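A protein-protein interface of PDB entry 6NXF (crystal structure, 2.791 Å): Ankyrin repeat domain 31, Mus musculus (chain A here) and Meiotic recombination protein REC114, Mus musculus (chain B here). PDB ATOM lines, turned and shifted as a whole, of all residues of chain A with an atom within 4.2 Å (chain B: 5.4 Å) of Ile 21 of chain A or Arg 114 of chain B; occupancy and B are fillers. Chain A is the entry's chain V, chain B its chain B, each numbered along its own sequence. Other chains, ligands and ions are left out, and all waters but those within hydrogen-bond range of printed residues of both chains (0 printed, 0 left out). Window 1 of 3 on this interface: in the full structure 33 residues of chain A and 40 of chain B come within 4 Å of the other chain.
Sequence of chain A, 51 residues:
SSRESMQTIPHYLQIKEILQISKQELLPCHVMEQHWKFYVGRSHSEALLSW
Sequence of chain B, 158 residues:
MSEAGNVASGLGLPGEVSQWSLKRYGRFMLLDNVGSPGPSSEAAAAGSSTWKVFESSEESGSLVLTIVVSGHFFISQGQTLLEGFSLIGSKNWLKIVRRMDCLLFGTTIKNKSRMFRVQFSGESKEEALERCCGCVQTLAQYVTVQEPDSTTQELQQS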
ATOM      1  N   LEU A  19      10.673   6.671  30.504  1.00  0.00           N
ATOM      2  CA  LEU A  19       9.643   5.720  30.106  1.00  0.00           C
ATOM      3  C   LEU A  19      10.210   4.848  28.991  1.00  0.00           C
ATOM      4  O   LEU A  19      10.238   5.241  27.827  1.00  0.00           O
ATOM      5  CB  LEU A  19       8.376   6.437  29.660  1.00  0.00           C
ATOM      6  CG  LEU A  19       7.283   5.458  29.193  1.00  0.00           C
ATOM      7  CD1 LEU A  19       6.925   4.502  30.319  1.00  0.00           C
ATOM      8  CD2 LEU A  19       6.059   6.190  28.684  1.00  0.00           C
ATOM      9  N   GLN A  20      10.653   3.655  29.362  1.00  0.00           N
ATOM     10  CA  GLN A  20      11.230   2.702  28.436  1.00  0.00           C
ATOM     11  C   GLN A  20      10.275   2.407  27.273  1.00  0.00           C
ATOM     12  O   GLN A  20       9.100   2.795  27.267  1.00  0.00           O
ATOM     13  CB  GLN A  20      11.605   1.427  29.184  1.00  0.00           C
ATOM     14  CG  GLN A  20      10.595   1.077  30.273  1.00  0.00           C
ATOM     15  CD  GLN A  20      10.913  -0.232  30.985  1.00  0.00           C
ATOM     16  OE1 GLN A  20      12.093  -0.569  31.188  1.00  0.00           O
ATOM     17  NE2 GLN A  20       9.860  -0.983  31.367  1.00  0.00           N
ATOM     18  N   ILE A  21      10.831   1.728  26.268  1.00  0.00           N
ATOM     19  CA  ILE A  21      10.166   1.445  25.005  1.00  0.00           C
ATOM     20  C   ILE A  21       9.463   0.090  25.117  1.00  0.00           C
ATOM     21  O   ILE A  21      10.092  -0.925  25.444  1.00  0.00           O
ATOM     22  CB  ILE A  21      11.197   1.461  23.866  1.00  0.00           C
ATOM     23  CG1 ILE A  21      11.011   2.684  22.973  1.00  0.00           C
ATOM     24  CG2 ILE A  21      11.124   0.184  23.013  1.00  0.00           C
ATOM     25  CD1 ILE A  21       9.874   2.442  22.020  1.00  0.00           C
ATOM     26  N   SER A  22       8.152   0.064  24.887  1.00  0.00           N
ATOM     27  CA  SER A  22       7.427  -1.202  24.979  1.00  0.00           C
ATOM     28  C   SER A  22       7.702  -2.090  23.761  1.00  0.00           C
ATOM     29  O   SER A  22       7.553  -1.653  22.615  1.00  0.00           O
ATOM     30  CB  SER A  22       5.927  -0.953  25.113  1.00  0.00           C
ATOM     31  OG  SER A  22       5.206  -2.175  25.023  1.00  0.00           O
ATOM     32  N   LYS A  23       8.076  -3.354  24.019  1.00  0.00           N
ATOM     33  CA  LYS A  23       8.404  -4.288  22.942  1.00  0.00           C
ATOM     34  C   LYS A  23       7.309  -4.329  21.884  1.00  0.00           C
ATOM     35  O   LYS A  23       7.588  -4.636  20.717  1.00  0.00           O
ATOM     36  CB  LYS A  23       8.666  -5.684  23.522  1.00  0.00           C
ATOM     37  N   GLU A  25       5.895  -1.615  20.793  1.00  0.00           N
ATOM     38  CA  GLU A  25       5.970  -0.415  19.969  1.00  0.00           C
ATOM     39  C   GLU A  25       6.953  -0.566  18.831  1.00  0.00           C
ATOM     40  O   GLU A  25       6.910   0.241  17.899  1.00  0.00           O
ATOM     41  CB  GLU A  25       6.370   0.802  20.793  1.00  0.00           C
ATOM     42  CG  GLU A  25       5.750   0.870  22.160  1.00  0.00           C
ATOM     43  CD  GLU A  25       6.235   2.080  22.981  1.00  0.00           C
ATOM     44  OE1 GLU A  25       6.031   2.090  24.228  1.00  0.00           O
ATOM     45  OE2 GLU A  25       6.811   3.017  22.367  1.00  0.00           O
ATOM     46  N   LEU A  26       7.823  -1.575  18.908  1.00  0.00           N
ATOM     47  CA  LEU A  26       8.784  -1.924  17.867  1.00  0.00           C
ATOM     48  C   LEU A  26       8.175  -2.930  16.888  1.00  0.00           C
ATOM     49  O   LEU A  26       8.012  -4.109  17.223  1.00  0.00           O
ATOM     50  CB  LEU A  26      10.033  -2.509  18.512  1.00  0.00           C
ATOM     51  CG  LEU A  26      10.784  -1.582  19.450  1.00  0.00           C
ATOM     52  CD1 LEU A  26      12.078  -2.227  19.954  1.00  0.00           C
ATOM     53  CD2 LEU A  26      11.073  -0.252  18.751  1.00  0.00           C
ATOM     54  N   LEU A  27       7.867  -2.475  15.678  1.00  0.00           N
ATOM     55  CA  LEU A  27       7.334  -3.285  14.595  1.00  0.00           C
ATOM     56  C   LEU A  27       8.362  -3.495  13.483  1.00  0.00           C
ATOM     57  O   LEU A  27       9.259  -2.662  13.274  1.00  0.00           O
ATOM     58  CB  LEU A  27       6.082  -2.626  14.005  1.00  0.00           C
ATOM     59  CG  LEU A  27       5.619  -1.310  14.631  1.00  0.00           C
ATOM     60  CD1 LEU A  27       6.113  -0.029  13.904  1.00  0.00           C
ATOM     61  CD2 LEU A  27       4.118  -1.379  14.670  1.00  0.00           C
ATOM     62  N   TYR B  25       0.804  13.831  23.073  1.00  0.00           N
ATOM     63  CA  TYR B  25       1.893  13.094  22.440  1.00  0.00           C
ATOM     64  C   TYR B  25       1.487  11.631  22.498  1.00  0.00           C
ATOM     65  O   TYR B  25       0.901  11.188  23.498  1.00  0.00           O
ATOM     66  CB  TYR B  25       3.250  13.335  23.145  1.00  0.00           C
ATOM     67  CG  TYR B  25       4.218  12.147  23.215  1.00  0.00           C
ATOM     68  CD1 TYR B  25       5.198  11.953  22.253  1.00  0.00           C
ATOM     69  CD2 TYR B  25       4.166  11.238  24.273  1.00  0.00           C
ATOM     70  CE1 TYR B  25       6.083  10.872  22.323  1.00  0.00           C
ATOM     71  CE2 TYR B  25       5.041  10.151  24.348  1.00  0.00           C
ATOM     72  CZ  TYR B  25       6.002   9.971  23.372  1.00  0.00           C
ATOM     73  OH  TYR B  25       6.876   8.895  23.458  1.00  0.00           O
ATOM     74  N   ARG B  27       2.334   7.368  21.305  1.00  0.00           N
ATOM     75  CA  ARG B  27       3.180   6.287  20.823  1.00  0.00           C
ATOM     76  C   ARG B  27       2.327   5.290  20.057  1.00  0.00           C
ATOM     77  O   ARG B  27       1.255   4.912  20.527  1.00  0.00           O
ATOM     78  CB  ARG B  27       3.866   5.564  21.972  1.00  0.00           C
ATOM     79  CG  ARG B  27       4.962   6.316  22.630  1.00  0.00           C
ATOM     80  CD  ARG B  27       5.575   5.452  23.723  1.00  0.00           C
ATOM     81  NE  ARG B  27       6.690   6.133  24.357  1.00  0.00           N
ATOM     82  CZ  ARG B  27       7.527   5.545  25.197  1.00  0.00           C
ATOM     83  NH1 ARG B  27       7.375   4.266  25.483  1.00  0.00           N
ATOM     84  NH2 ARG B  27       8.518   6.239  25.737  1.00  0.00           N
ATOM     85  N   LEU B  82      10.227  11.013  27.726  1.00  0.00           N
ATOM     86  CA  LEU B  82       9.422  10.247  26.785  1.00  0.00           C
ATOM     87  C   LEU B  82      10.170   9.892  25.502  1.00  0.00           C
ATOM     88  O   LEU B  82      10.124   8.737  25.071  1.00  0.00           O
ATOM     89  CB  LEU B  82       8.151  11.037  26.459  1.00  0.00           C
ATOM     90  CG  LEU B  82       7.291  11.275  27.703  1.00  0.00           C
ATOM     91  CD1 LEU B  82       6.105  12.166  27.366  1.00  0.00           C
ATOM     92  CD2 LEU B  82       6.850   9.954  28.349  1.00  0.00           C
ATOM     93  N   GLU B  83      10.854  10.859  24.882  1.00  0.00           N
ATOM     94  CA  GLU B  83      11.673  10.627  23.704  1.00  0.00           C
ATOM     95  C   GLU B  83      13.055  11.225  23.894  1.00  0.00           C
ATOM     96  O   GLU B  83      13.201  12.324  24.436  1.00  0.00           O
ATOM     97  CB  GLU B  83      11.050  11.234  22.453  1.00  0.00           C
ATOM     98  CG  GLU B  83       9.788  10.511  21.955  1.00  0.00           C
ATOM     99  CD  GLU B  83      10.001   9.016  21.720  1.00  0.00           C
ATOM    100  OE1 GLU B  83      11.168   8.585  21.514  1.00  0.00           O
ATOM    101  OE2 GLU B  83       8.983   8.274  21.755  1.00  0.00           O
ATOM    102  N   PHE B 105       6.514  11.227  13.657  1.00  0.00           N
ATOM    103  CA  PHE B 105       7.905  10.804  13.618  1.00  0.00           C
ATOM    104  C   PHE B 105       7.962   9.302  13.392  1.00  0.00           C
ATOM    105  O   PHE B 105       7.226   8.546  14.025  1.00  0.00           O
ATOM    106  CB  PHE B 105       8.640  11.152  14.919  1.00  0.00           C
ATOM    107  CG  PHE B 105       8.791  12.633  15.180  1.00  0.00           C
ATOM    108  CD1 PHE B 105       7.693  13.430  15.457  1.00  0.00           C
ATOM    109  CD2 PHE B 105      10.050  13.220  15.205  1.00  0.00           C
ATOM    110  CE1 PHE B 105       7.852  14.801  15.728  1.00  0.00           C
ATOM    111  CE2 PHE B 105      10.210  14.582  15.481  1.00  0.00           C
ATOM    112  CZ  PHE B 105       9.107  15.368  15.736  1.00  0.00           C
ATOM    113  N   GLY B 106       8.833   8.871  12.489  1.00  0.00           N
ATOM    114  CA  GLY B 106       9.027   7.453  12.265  1.00  0.00           C
ATOM    115  C   GLY B 106      10.501   7.177  12.304  1.00  0.00           C
ATOM    116  O   GLY B 106      11.277   7.854  11.628  1.00  0.00           O
ATOM    117  N   THR B 107      10.922   6.227  13.117  1.00  0.00           N
ATOM    118  CA  THR B 107      12.340   6.002  13.340  1.00  0.00           C
ATOM    119  C   THR B 107      12.641   4.543  13.070  1.00  0.00           C
ATOM    120  O   THR B 107      11.983   3.661  13.631  1.00  0.00           O
ATOM    121  CB  THR B 107      12.749   6.362  14.777  1.00  0.00           C
ATOM    122  OG1 THR B 107      12.970   5.163  15.535  1.00  0.00           O
ATOM    123  CG2 THR B 107      11.649   7.130  15.444  1.00  0.00           C
ATOM    124  N   THR B 108      13.629   4.282  12.232  1.00  0.00           N
ATOM    125  CA  THR B 108      14.112   2.926  12.038  1.00  0.00           C
ATOM    126  C   THR B 108      15.463   2.814  12.729  1.00  0.00           C
ATOM    127  O   THR B 108      16.273   3.739  12.642  1.00  0.00           O
ATOM    128  CB  THR B 108      14.191   2.604  10.546  1.00  0.00           C
ATOM    129  OG1 THR B 108      12.878   2.741   9.964  1.00  0.00           O
ATOM    130  CG2 THR B 108      14.712   1.193  10.322  1.00  0.00           C
ATOM    131  N   LYS B 112      14.338  -2.180  13.240  1.00  0.00           N
ATOM    132  CA  LYS B 112      13.067  -2.185  13.968  1.00  0.00           C
ATOM    133  C   LYS B 112      12.528  -0.764  13.970  1.00  0.00           C
ATOM    134  O   LYS B 112      13.124   0.106  14.603  1.00  0.00           O
ATOM    135  CB  LYS B 112      13.258  -2.671  15.393  1.00  0.00           C
ATOM    136  CG  LYS B 112      13.456  -4.147  15.499  1.00  0.00           C
ATOM    137  CD  LYS B 112      12.229  -4.876  15.027  1.00  0.00           C
ATOM    138  CE  LYS B 112      12.366  -6.343  15.370  1.00  0.00           C
ATOM    139  NZ  LYS B 112      12.687  -6.526  16.829  1.00  0.00           N
ATOM    140  N   SER B 113      11.422  -0.505  13.293  1.00  0.00           N
ATOM    141  CA  SER B 113      10.962   0.873  13.242  1.00  0.00           C
ATOM    142  C   SER B 113       9.809   1.117  14.227  1.00  0.00           C
ATOM    143  O   SER B 113       9.335   0.213  14.920  1.00  0.00           O
ATOM    144  CB  SER B 113      10.553   1.248  11.818  1.00  0.00           C
ATOM    145  OG  SER B 113       9.321   0.651  11.527  1.00  0.00           O
ATOM    146  N   ARG B 114       9.390   2.378  14.320  1.00  0.00           N
ATOM    147  CA  ARG B 114       8.344   2.764  15.263  1.00  0.00           C
ATOM    148  C   ARG B 114       7.923   4.201  15.001  1.00  0.00           C
ATOM    149  O   ARG B 114       8.620   4.957  14.318  1.00  0.00           O
ATOM    150  CB  ARG B 114       8.804   2.606  16.716  1.00  0.00           C
ATOM    151  CG  ARG B 114       9.304   3.849  17.373  1.00  0.00           C
ATOM    152  CD  ARG B 114      10.070   3.469  18.611  1.00  0.00           C
ATOM    153  NE  ARG B 114       9.588   4.223  19.756  1.00  0.00           N
ATOM    154  CZ  ARG B 114      10.056   5.404  20.144  1.00  0.00           C
ATOM    155  NH1 ARG B 114      11.040   6.002  19.467  1.00  0.00           N
ATOM    156  NH2 ARG B 114       9.529   5.983  21.213  1.00  0.00           N
ATOM    157  N   MET B 115       6.777   4.568  15.559  1.00  0.00           N
ATOM    158  CA  MET B 115       6.247   5.907  15.373  1.00  0.00           C
ATOM    159  C   MET B 115       5.798   6.606  16.663  1.00  0.00           C
ATOM    160  O   MET B 115       5.456   5.957  17.652  1.00  0.00           O
ATOM    161  CB  MET B 115       5.061   5.866  14.425  1.00  0.00           C
ATOM    162  CG  MET B 115       5.378   5.997  12.965  1.00  0.00           C
ATOM    163  SD  MET B 115       3.844   5.406  11.882  1.00  0.00           S
ATOM    164  CE  MET B 115       3.712   3.529  12.480  1.00  0.00           C
ATOM    165  N   PHE B 116       5.786   7.937  16.634  1.00  0.00           N
ATOM    166  CA  PHE B 116       5.141   8.728  17.670  1.00  0.00           C
ATOM    167  C   PHE B 116       4.779  10.067  17.056  1.00  0.00           C
ATOM    168  O   PHE B 116       5.435  10.518  16.118  1.00  0.00           O
ATOM    169  CB  PHE B 116       6.016   8.901  18.923  1.00  0.00           C
ATOM    170  CG  PHE B 116       7.308   9.646  18.690  1.00  0.00           C
ATOM    171  CD1 PHE B 116       7.347  11.031  18.713  1.00  0.00           C
ATOM    172  CD2 PHE B 116       8.507   8.948  18.480  1.00  0.00           C
ATOM    173  CE1 PHE B 116       8.551  11.700  18.508  1.00  0.00           C
ATOM    174  CE2 PHE B 116       9.713   9.611  18.271  1.00  0.00           C
ATOM    175  CZ  PHE B 116       9.739  10.985  18.288  1.00  0.00           C
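NH1 of Arg 27 of chain B is in salt-bridge range of OE1 of Glu 25 of chain A (2.8 Å). NH1 of Arg 27 of chain B is in hydrogen-bond range of O of Gln 20 of chain A, 2.9 Å away. The guanidinium group of Arg 27 of chain B lies within hydrogen-bond range of the backbone carbonyl oxygen of Leu 19 of chain A, at 2.9 Å. O of Leu 27 of chain A is in hydrogen-bond range of N of Ser 113 of chain B, at 3.1 Å. The side-chain carboxylate (OE2) of Glu 25 of chain A lies within salt-bridge range of the guanidinium group (NE) of Arg 114 of chain B.
N of Thr 107 of chain B sits at hydrogen-bond distance from O of Arg 114 of chain B. OE2 of Glu 83 of chain B lies within salt-bridge range of NH2 of Arg 114 of chain B. OH of Tyr 25 of chain B is in hydrogen-bond range of NE of Arg 27 of chain B (2.9 Å). OE1 of Glu 25 of chain A is in hydrogen-bond range of N of Ser 22 of chain A. The backbone carbonyl oxygen (O) of Leu 82 of chain B lies within hydrogen-bond range of the guanidinium group (NH2) of Arg 27 of chain B, at 3.0 Å.
Leu 19 of chain A touches Leu 82 of chain B (CD2 to CD2, 3.9 Å). Ile 21 of chain A touches Arg 27 of chain B. Arg 114 of chain B touches Ile 21 of chain A. Glu 25 of chain A touches Ser 113 of chain B (O to O, 3.8 Å). Leu 26 of chain A touches Ser 113 of chain B. Leu 26 of chain A touches Arg 114 of chain B (CD2 to CD, 3.9 Å). O of Leu 27 of chain A touches C of Lys 112 of chain B (3.8 Å). Arg 114 of chain B touches Leu 27 of chain A.
Of the printed residues of chain B, Gln 20 of chain A touches Arg 27 (2.9 Å). Of the printed residues of chain B, Leu 27 of chain A touches Lys 112, Ser 113 and Arg 114. Printed residues of chain A within 4 Å of Arg 27 of chain B: Leu 19 (2.9 Å), Gln 20 (2.9 Å), Ile 21 (3.997 Å) and Glu 25 (2.8 Å). Printed residues of chain A within 4 Å of Leu 82 of chain B: Leu 19 (3.9 Å). Of the printed residues of chain A, Lys 112 of chain B touches Leu 27. Of chain A, only Ile 21 (2.9 Å), Glu 25 (3.3 Å), Leu 26 (3.9 Å) and Leu 27 (3.8 Å) come within 4 Å of Arg 114 of chain B. The nearest printed residue of chain B that does not touch Ile 21 of chain A is Glu 83 of chain B (5.9 Å). The nearest printed residue of chain A that does not touch Arg 114 of chain B is Leu 19 of chain A (6.7 Å).
Hydrophobic or aromatic side chains of chain B within 4 Å of the printed part of chain A: Leu 82. Hydrophobic or aromatic side chains of chain A within 4 Å of the printed part of chain B: Leu 19, Ile 21, Leu 26 and Leu 27. Among the printed residues, 13 pairs touch across the chains. Among the printed residues, Asp or Glu carboxylates within 4 Å of a Lys or Arg side-chain nitrogen of the other chain: Glu 25 of chain A with Arg 27 of chain B (2.8 Å) and Glu 25 of chain A with Arg 114 of chain B (3.998 Å).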
